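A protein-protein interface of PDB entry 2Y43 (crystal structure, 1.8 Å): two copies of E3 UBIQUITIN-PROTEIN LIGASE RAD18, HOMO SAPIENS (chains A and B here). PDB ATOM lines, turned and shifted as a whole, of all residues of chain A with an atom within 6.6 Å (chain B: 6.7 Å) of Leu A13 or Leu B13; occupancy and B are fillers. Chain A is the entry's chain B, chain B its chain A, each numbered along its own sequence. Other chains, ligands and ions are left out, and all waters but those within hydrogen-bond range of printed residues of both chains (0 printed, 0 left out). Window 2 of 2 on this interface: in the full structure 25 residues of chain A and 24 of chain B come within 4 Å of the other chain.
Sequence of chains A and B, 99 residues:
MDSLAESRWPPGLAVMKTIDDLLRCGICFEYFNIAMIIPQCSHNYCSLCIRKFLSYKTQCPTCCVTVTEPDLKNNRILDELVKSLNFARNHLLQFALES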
ATOM      1  N   TRP A   9      11.067 -10.937 -26.281  1.00  0.00           N
ATOM      2  CA  TRP A   9      11.416 -11.926 -25.263  1.00  0.00           C
ATOM      3  C   TRP A   9      10.355 -12.015 -24.167  1.00  0.00           C
ATOM      4  O   TRP A   9       9.519 -11.115 -24.047  1.00  0.00           O
ATOM      5  CB  TRP A   9      12.814 -11.607 -24.700  1.00  0.00           C
ATOM      6  CG  TRP A   9      13.882 -11.676 -25.757  1.00  0.00           C
ATOM      7  CD1 TRP A   9      14.055 -10.819 -26.808  1.00  0.00           C
ATOM      8  CD2 TRP A   9      14.920 -12.667 -25.878  1.00  0.00           C
ATOM      9  NE1 TRP A   9      15.122 -11.214 -27.571  1.00  0.00           N
ATOM     10  CE2 TRP A   9      15.670 -12.344 -27.026  1.00  0.00           C
ATOM     11  CE3 TRP A   9      15.274 -13.799 -25.134  1.00  0.00           C
ATOM     12  CZ2 TRP A   9      16.769 -13.110 -27.451  1.00  0.00           C
ATOM     13  CZ3 TRP A   9      16.373 -14.562 -25.551  1.00  0.00           C
ATOM     14  CH2 TRP A   9      17.100 -14.214 -26.700  1.00  0.00           C
ATOM     15  N   PRO A  10      10.352 -13.113 -23.378  1.00  0.00           N
ATOM     16  CA  PRO A  10       9.372 -13.166 -22.305  1.00  0.00           C
ATOM     17  C   PRO A  10       9.612 -12.032 -21.310  1.00  0.00           C
ATOM     18  O   PRO A  10      10.692 -11.421 -21.339  1.00  0.00           O
ATOM     19  CB  PRO A  10       9.618 -14.535 -21.649  1.00  0.00           C
ATOM     20  CG  PRO A  10      10.940 -14.977 -22.117  1.00  0.00           C
ATOM     21  CD  PRO A  10      11.128 -14.364 -23.472  1.00  0.00           C
ATOM     22  N   PRO A  11       8.608 -11.732 -20.464  1.00  0.00           N
ATOM     23  CA  PRO A  11       8.709 -10.659 -19.478  1.00  0.00           C
ATOM     24  C   PRO A  11      10.019 -10.651 -18.692  1.00  0.00           C
ATOM     25  O   PRO A  11      10.443 -11.679 -18.146  1.00  0.00           O
ATOM     26  CB  PRO A  11       7.531 -10.941 -18.543  1.00  0.00           C
ATOM     27  CG  PRO A  11       6.500 -11.514 -19.443  1.00  0.00           C
ATOM     28  CD  PRO A  11       7.250 -12.316 -20.483  1.00  0.00           C
ATOM     29  N   GLY A  12      10.647  -9.483 -18.655  1.00  0.00           N
ATOM     30  CA  GLY A  12      11.827  -9.272 -17.835  1.00  0.00           C
ATOM     31  C   GLY A  12      13.124  -9.583 -18.538  1.00  0.00           C
ATOM     32  O   GLY A  12      14.143  -9.751 -17.880  1.00  0.00           O
ATOM     33  N   LEU A  13      13.086  -9.653 -19.869  1.00  0.00           N
ATOM     34  CA  LEU A  13      14.286  -9.890 -20.666  1.00  0.00           C
ATOM     35  C   LEU A  13      14.535  -8.748 -21.648  1.00  0.00           C
ATOM     36  O   LEU A  13      15.113  -8.955 -22.710  1.00  0.00           O
ATOM     37  CB  LEU A  13      14.220 -11.237 -21.403  1.00  0.00           C
ATOM     38  CG  LEU A  13      14.237 -12.527 -20.565  1.00  0.00           C
ATOM     39  CD1 LEU A  13      14.228 -13.731 -21.498  1.00  0.00           C
ATOM     40  CD2 LEU A  13      15.464 -12.582 -19.663  1.00  0.00           C
ATOM     41  N   ALA A  14      14.098  -7.545 -21.275  1.00  0.00           N
ATOM     42  CA  ALA A  14      14.287  -6.354 -22.114  1.00  0.00           C
ATOM     43  C   ALA A  14      15.763  -6.126 -22.439  1.00  0.00           C
ATOM     44  O   ALA A  14      16.104  -5.642 -23.520  1.00  0.00           O
ATOM     45  CB  ALA A  14      13.688  -5.129 -21.432  1.00  0.00           C
ATOM     46  N   VAL A  15      16.643  -6.510 -21.515  1.00  0.00           N
ATOM     47  CA  VAL A  15      18.091  -6.375 -21.716  1.00  0.00           C
ATOM     48  C   VAL A  15      18.597  -7.123 -22.960  1.00  0.00           C
ATOM     49  O   VAL A  15      19.630  -6.763 -23.543  1.00  0.00           O
ATOM     50  CB  VAL A  15      18.895  -6.775 -20.433  1.00  0.00           C
ATOM     51  CG1 VAL A  15      18.975  -8.289 -20.278  1.00  0.00           C
ATOM     52  CG2 VAL A  15      20.301  -6.147 -20.456  1.00  0.00           C
ATOM     53  N   MET A  16      17.862  -8.144 -23.399  1.00  0.00           N
ATOM     54  CA  MET A  16      18.276  -8.886 -24.595  1.00  0.00           C
ATOM     55  C   MET A  16      18.247  -8.060 -25.890  1.00  0.00           C
ATOM     56  O   MET A  16      18.867  -8.453 -26.872  1.00  0.00           O
ATOM     57  CB  MET A  16      17.492 -10.186 -24.756  1.00  0.00           C
ATOM     58  CG  MET A  16      17.673 -11.140 -23.580  1.00  0.00           C
ATOM     59  SD  MET A  16      19.428 -11.556 -23.386  1.00  0.00           S
ATOM     60  CE  MET A  16      19.769 -12.287 -24.978  1.00  0.00           C
ATOM     61  N   LYS A  17      17.548  -6.925 -25.886  1.00  0.00           N
ATOM     62  CA  LYS A  17      17.458  -6.103 -27.103  1.00  0.00           C
ATOM     63  C   LYS A  17      18.842  -5.704 -27.661  1.00  0.00           C
ATOM     64  O   LYS A  17      19.058  -5.714 -28.873  1.00  0.00           O
ATOM     65  CB  LYS A  17      16.556  -4.875 -26.892  1.00  0.00           C
ATOM     66  CG  LYS A  17      16.363  -4.059 -28.162  1.00  0.00           C
ATOM     67  CD  LYS A  17      15.407  -2.922 -27.977  1.00  0.00           C
ATOM     68  CE  LYS A  17      15.423  -2.005 -29.181  1.00  0.00           C
ATOM     69  NZ  LYS A  17      16.735  -1.331 -29.308  1.00  0.00           N
ATOM     70  N   LEU A  92      12.534 -20.045 -24.721  1.00  0.00           N
ATOM     71  CA  LEU A  92      12.101 -19.287 -23.533  1.00  0.00           C
ATOM     72  C   LEU A  92      10.628 -18.894 -23.600  1.00  0.00           C
ATOM     73  O   LEU A  92       9.896 -19.007 -22.600  1.00  0.00           O
ATOM     74  CB  LEU A  92      12.976 -18.040 -23.334  1.00  0.00           C
ATOM     75  CG  LEU A  92      14.466 -18.299 -23.079  1.00  0.00           C
ATOM     76  CD1 LEU A  92      15.274 -17.021 -23.202  1.00  0.00           C
ATOM     77  CD2 LEU A  92      14.686 -18.952 -21.726  1.00  0.00           C
ATOM     78  N   TRP B   9      23.961 -18.499 -15.827  1.00  0.00           N
ATOM     79  CA  TRP B   9      22.554 -18.191 -16.001  1.00  0.00           C
ATOM     80  C   TRP B   9      21.706 -19.004 -15.042  1.00  0.00           C
ATOM     81  O   TRP B   9      22.065 -20.144 -14.732  1.00  0.00           O
ATOM     82  CB  TRP B   9      22.159 -18.509 -17.437  1.00  0.00           C
ATOM     83  CG  TRP B   9      22.986 -17.774 -18.430  1.00  0.00           C
ATOM     84  CD1 TRP B   9      24.123 -18.213 -19.049  1.00  0.00           C
ATOM     85  CD2 TRP B   9      22.750 -16.450 -18.911  1.00  0.00           C
ATOM     86  NE1 TRP B   9      24.603 -17.239 -19.896  1.00  0.00           N
ATOM     87  CE2 TRP B   9      23.781 -16.145 -19.823  1.00  0.00           C
ATOM     88  CE3 TRP B   9      21.766 -15.485 -18.651  1.00  0.00           C
ATOM     89  CZ2 TRP B   9      23.849 -14.921 -20.491  1.00  0.00           C
ATOM     90  CZ3 TRP B   9      21.835 -14.267 -19.314  1.00  0.00           C
ATOM     91  CH2 TRP B   9      22.863 -14.003 -20.231  1.00  0.00           C
ATOM     92  N   PRO B  10      20.587 -18.421 -14.555  1.00  0.00           N
ATOM     93  CA  PRO B  10      19.648 -19.192 -13.744  1.00  0.00           C
ATOM     94  C   PRO B  10      18.969 -20.248 -14.616  1.00  0.00           C
ATOM     95  O   PRO B  10      18.996 -20.122 -15.844  1.00  0.00           O
ATOM     96  CB  PRO B  10      18.633 -18.139 -13.272  1.00  0.00           C
ATOM     97  CG  PRO B  10      18.665 -17.101 -14.324  1.00  0.00           C
ATOM     98  CD  PRO B  10      20.095 -17.055 -14.818  1.00  0.00           C
ATOM     99  N   PRO B  11      18.388 -21.294 -13.996  1.00  0.00           N
ATOM    100  CA  PRO B  11      17.806 -22.407 -14.746  1.00  0.00           C
ATOM    101  C   PRO B  11      16.837 -21.966 -15.838  1.00  0.00           C
ATOM    102  O   PRO B  11      16.900 -22.486 -16.952  1.00  0.00           O
ATOM    103  CB  PRO B  11      17.077 -23.202 -13.669  1.00  0.00           C
ATOM    104  CG  PRO B  11      17.908 -22.986 -12.464  1.00  0.00           C
ATOM    105  CD  PRO B  11      18.346 -21.543 -12.545  1.00  0.00           C
ATOM    106  N   GLY B  12      15.967 -21.004 -15.519  1.00  0.00           N
ATOM    107  CA  GLY B  12      15.069 -20.396 -16.498  1.00  0.00           C
ATOM    108  C   GLY B  12      15.757 -20.015 -17.802  1.00  0.00           C
ATOM    109  O   GLY B  12      15.137 -20.070 -18.867  1.00  0.00           O
ATOM    110  N   LEU B  13      17.043 -19.670 -17.717  1.00  0.00           N
ATOM    111  CA  LEU B  13      17.807 -19.148 -18.855  1.00  0.00           C
ATOM    112  C   LEU B  13      19.026 -20.012 -19.206  1.00  0.00           C
ATOM    113  O   LEU B  13      19.965 -19.542 -19.847  1.00  0.00           O
ATOM    114  CB  LEU B  13      18.262 -17.704 -18.583  1.00  0.00           C
ATOM    115  CG  LEU B  13      17.200 -16.633 -18.301  1.00  0.00           C
ATOM    116  CD1 LEU B  13      17.852 -15.322 -17.836  1.00  0.00           C
ATOM    117  CD2 LEU B  13      16.340 -16.383 -19.527  1.00  0.00           C
ATOM    118  N   ALA B  14      18.997 -21.277 -18.794  1.00  0.00           N
ATOM    119  CA  ALA B  14      20.124 -22.183 -19.011  1.00  0.00           C
ATOM    120  C   ALA B  14      20.549 -22.230 -20.479  1.00  0.00           C
ATOM    121  O   ALA B  14      21.737 -22.318 -20.795  1.00  0.00           O
ATOM    122  CB  ALA B  14      19.774 -23.573 -18.505  1.00  0.00           C
ATOM    123  N   VAL B  15      19.569 -22.135 -21.375  1.00  0.00           N
ATOM    124  CA  VAL B  15      19.830 -22.186 -22.823  1.00  0.00           C
ATOM    125  C   VAL B  15      20.840 -21.130 -23.305  1.00  0.00           C
ATOM    126  O   VAL B  15      21.522 -21.325 -24.323  1.00  0.00           O
ATOM    127  CB  VAL B  15      18.486 -22.174 -23.642  1.00  0.00           C
ATOM    128  CG1 VAL B  15      17.669 -20.876 -23.396  1.00  0.00           C
ATOM    129  CG2 VAL B  15      18.738 -22.420 -25.120  1.00  0.00           C
ATOM    130  N   MET B  16      20.949 -20.025 -22.567  1.00  0.00           N
ATOM    131  CA  MET B  16      21.890 -18.955 -22.890  1.00  0.00           C
ATOM    132  C   MET B  16      23.344 -19.404 -22.845  1.00  0.00           C
ATOM    133  O   MET B  16      24.218 -18.742 -23.393  1.00  0.00           O
ATOM    134  CB  MET B  16      21.687 -17.768 -21.952  1.00  0.00           C
ATOM    135  CG  MET B  16      20.334 -17.090 -22.107  1.00  0.00           C
ATOM    136  SD  MET B  16      20.043 -16.474 -23.779  1.00  0.00           S
ATOM    137  CE  MET B  16      21.306 -15.200 -23.856  1.00  0.00           C
ATOM    138  N   LYS B  17      23.603 -20.521 -22.177  1.00  0.00           N
ATOM    139  CA  LYS B  17      24.941 -21.096 -22.186  1.00  0.00           C
ATOM    140  C   LYS B  17      25.429 -21.358 -23.609  1.00  0.00           C
ATOM    141  O   LYS B  17      26.634 -21.319 -23.865  1.00  0.00           O
ATOM    142  CB  LYS B  17      25.003 -22.381 -21.354  1.00  0.00           C
ATOM    143  CG  LYS B  17      26.431 -22.796 -21.046  1.00  0.00           C
ATOM    144  CD  LYS B  17      26.588 -24.297 -20.983  1.00  0.00           C
ATOM    145  CE  LYS B  17      27.850 -24.654 -20.211  1.00  0.00           C
ATOM    146  NZ  LYS B  17      27.605 -25.850 -19.337  1.00  0.00           N
ATOM    147  N   ALA B  88      24.003  -8.274 -19.621  1.00  0.00           N
ATOM    148  CA  ALA B  88      22.747  -9.009 -19.537  1.00  0.00           C
ATOM    149  C   ALA B  88      22.844 -10.078 -18.462  1.00  0.00           C
ATOM    150  O   ALA B  88      21.987 -10.146 -17.580  1.00  0.00           O
ATOM    151  CB  ALA B  88      22.411  -9.650 -20.891  1.00  0.00           C
ATOM    152  N   LEU B  92      20.677 -10.553 -14.863  1.00  0.00           N
ATOM    153  CA  LEU B  92      19.668 -11.606 -14.968  1.00  0.00           C
ATOM    154  C   LEU B  92      19.937 -12.790 -14.047  1.00  0.00           C
ATOM    155  O   LEU B  92      19.319 -13.849 -14.209  1.00  0.00           O
ATOM    156  CB  LEU B  92      19.550 -12.099 -16.413  1.00  0.00           C
ATOM    157  CG  LEU B  92      18.916 -11.115 -17.400  1.00  0.00           C
ATOM    158  CD1 LEU B  92      19.008 -11.641 -18.817  1.00  0.00           C
ATOM    159  CD2 LEU B  92      17.468 -10.827 -16.992  1.00  0.00           C
ATOM    160  N   LEU B  93      20.843 -12.612 -13.083  1.00  0.00           N
ATOM    161  CA  LEU B  93      21.215 -13.693 -12.151  1.00  0.00           C
ATOM    162  C   LEU B  93      20.057 -14.211 -11.289  1.00  0.00           C
ATOM    163  O   LEU B  93      20.072 -15.368 -10.844  1.00  0.00           O
ATOM    164  CB  LEU B  93      22.381 -13.265 -11.251  1.00  0.00           C
ATOM    165  CG  LEU B  93      23.734 -12.943 -11.890  1.00  0.00           C
ATOM    166  CD1 LEU B  93      24.739 -12.537 -10.817  1.00  0.00           C
ATOM    167  CD2 LEU B  93      24.277 -14.114 -12.721  1.00  0.00           C
ATOM    168  N   PHE B  95      16.733 -13.996 -12.303  1.00  0.00           N
ATOM    169  CA  PHE B  95      15.561 -14.155 -13.174  1.00  0.00           C
ATOM    170  C   PHE B  95      14.807 -15.447 -12.850  1.00  0.00           C
ATOM    171  O   PHE B  95      15.392 -16.531 -12.829  1.00  0.00           O
ATOM    172  CB  PHE B  95      15.963 -14.129 -14.656  1.00  0.00           C
ATOM    173  CG  PHE B  95      14.808 -14.339 -15.609  1.00  0.00           C
ATOM    174  CD1 PHE B  95      13.986 -13.273 -15.981  1.00  0.00           C
ATOM    175  CD2 PHE B  95      14.540 -15.602 -16.130  1.00  0.00           C
ATOM    176  CE1 PHE B  95      12.915 -13.466 -16.863  1.00  0.00           C
ATOM    177  CE2 PHE B  95      13.470 -15.808 -17.008  1.00  0.00           C
ATOM    178  CZ  PHE B  95      12.660 -14.738 -17.379  1.00  0.00           C
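Leu A13 touches its own counterpart, Leu B13. Leu A13 touches Leu B92, and with the chains exchanged Leu A92 touches Leu B13. Val A15 touches Leu B92, and with the chains exchanged Leu A92 touches Val B15. Met B16 touches its own counterpart, Met A16. Positions printed for both chains: 9, 10, 11, 12, 13, 14, 15, 16, 17 and 92. Of the 11 pairs that touch across the chains among the printed residues, 8 have their exchanged pair printed and touching as well.
Phe B95 touches Pro A11 (CE1 to O, 3.3 Å). Leu B92 touches Gly A12 (CD2 to O, 3.6 Å). Leu A13 touches Leu B13. Leu B92 touches Leu A13 (CD1 to CD2, 3.8 Å). Phe B95 touches Leu A13. Val A15 touches Ala B88 (CG1 to CB, 3.7 Å). Met A16 touches Met B16. Gly B12 touches Leu A92 (O to CD2, 3.1 Å). Leu B13 touches Leu A92 (CD2 to CD2, 3.8 Å). Val B15 touches Leu A92.
Of the printed residues of chain B, Leu A13 touches Leu B13 (3.9 Å), Leu B92 (3.8 Å) and Phe B95 (3.9 Å). Leu B13 touches two residues of chain A. Of the printed residues of chain A, Phe B95 touches Pro A11 and Leu A13. Printed residues of chain B within 4 Å of Pro A11: Phe B95. The nearest printed residue of chain B that does not touch Met A16 is Ala B88 (4.3 Å).
Printed residues of chain B that touch a printed residue of chain A: Gly B12, Leu B13, Val B15, Met B16, Ala B88, Leu B92 and Phe B95.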
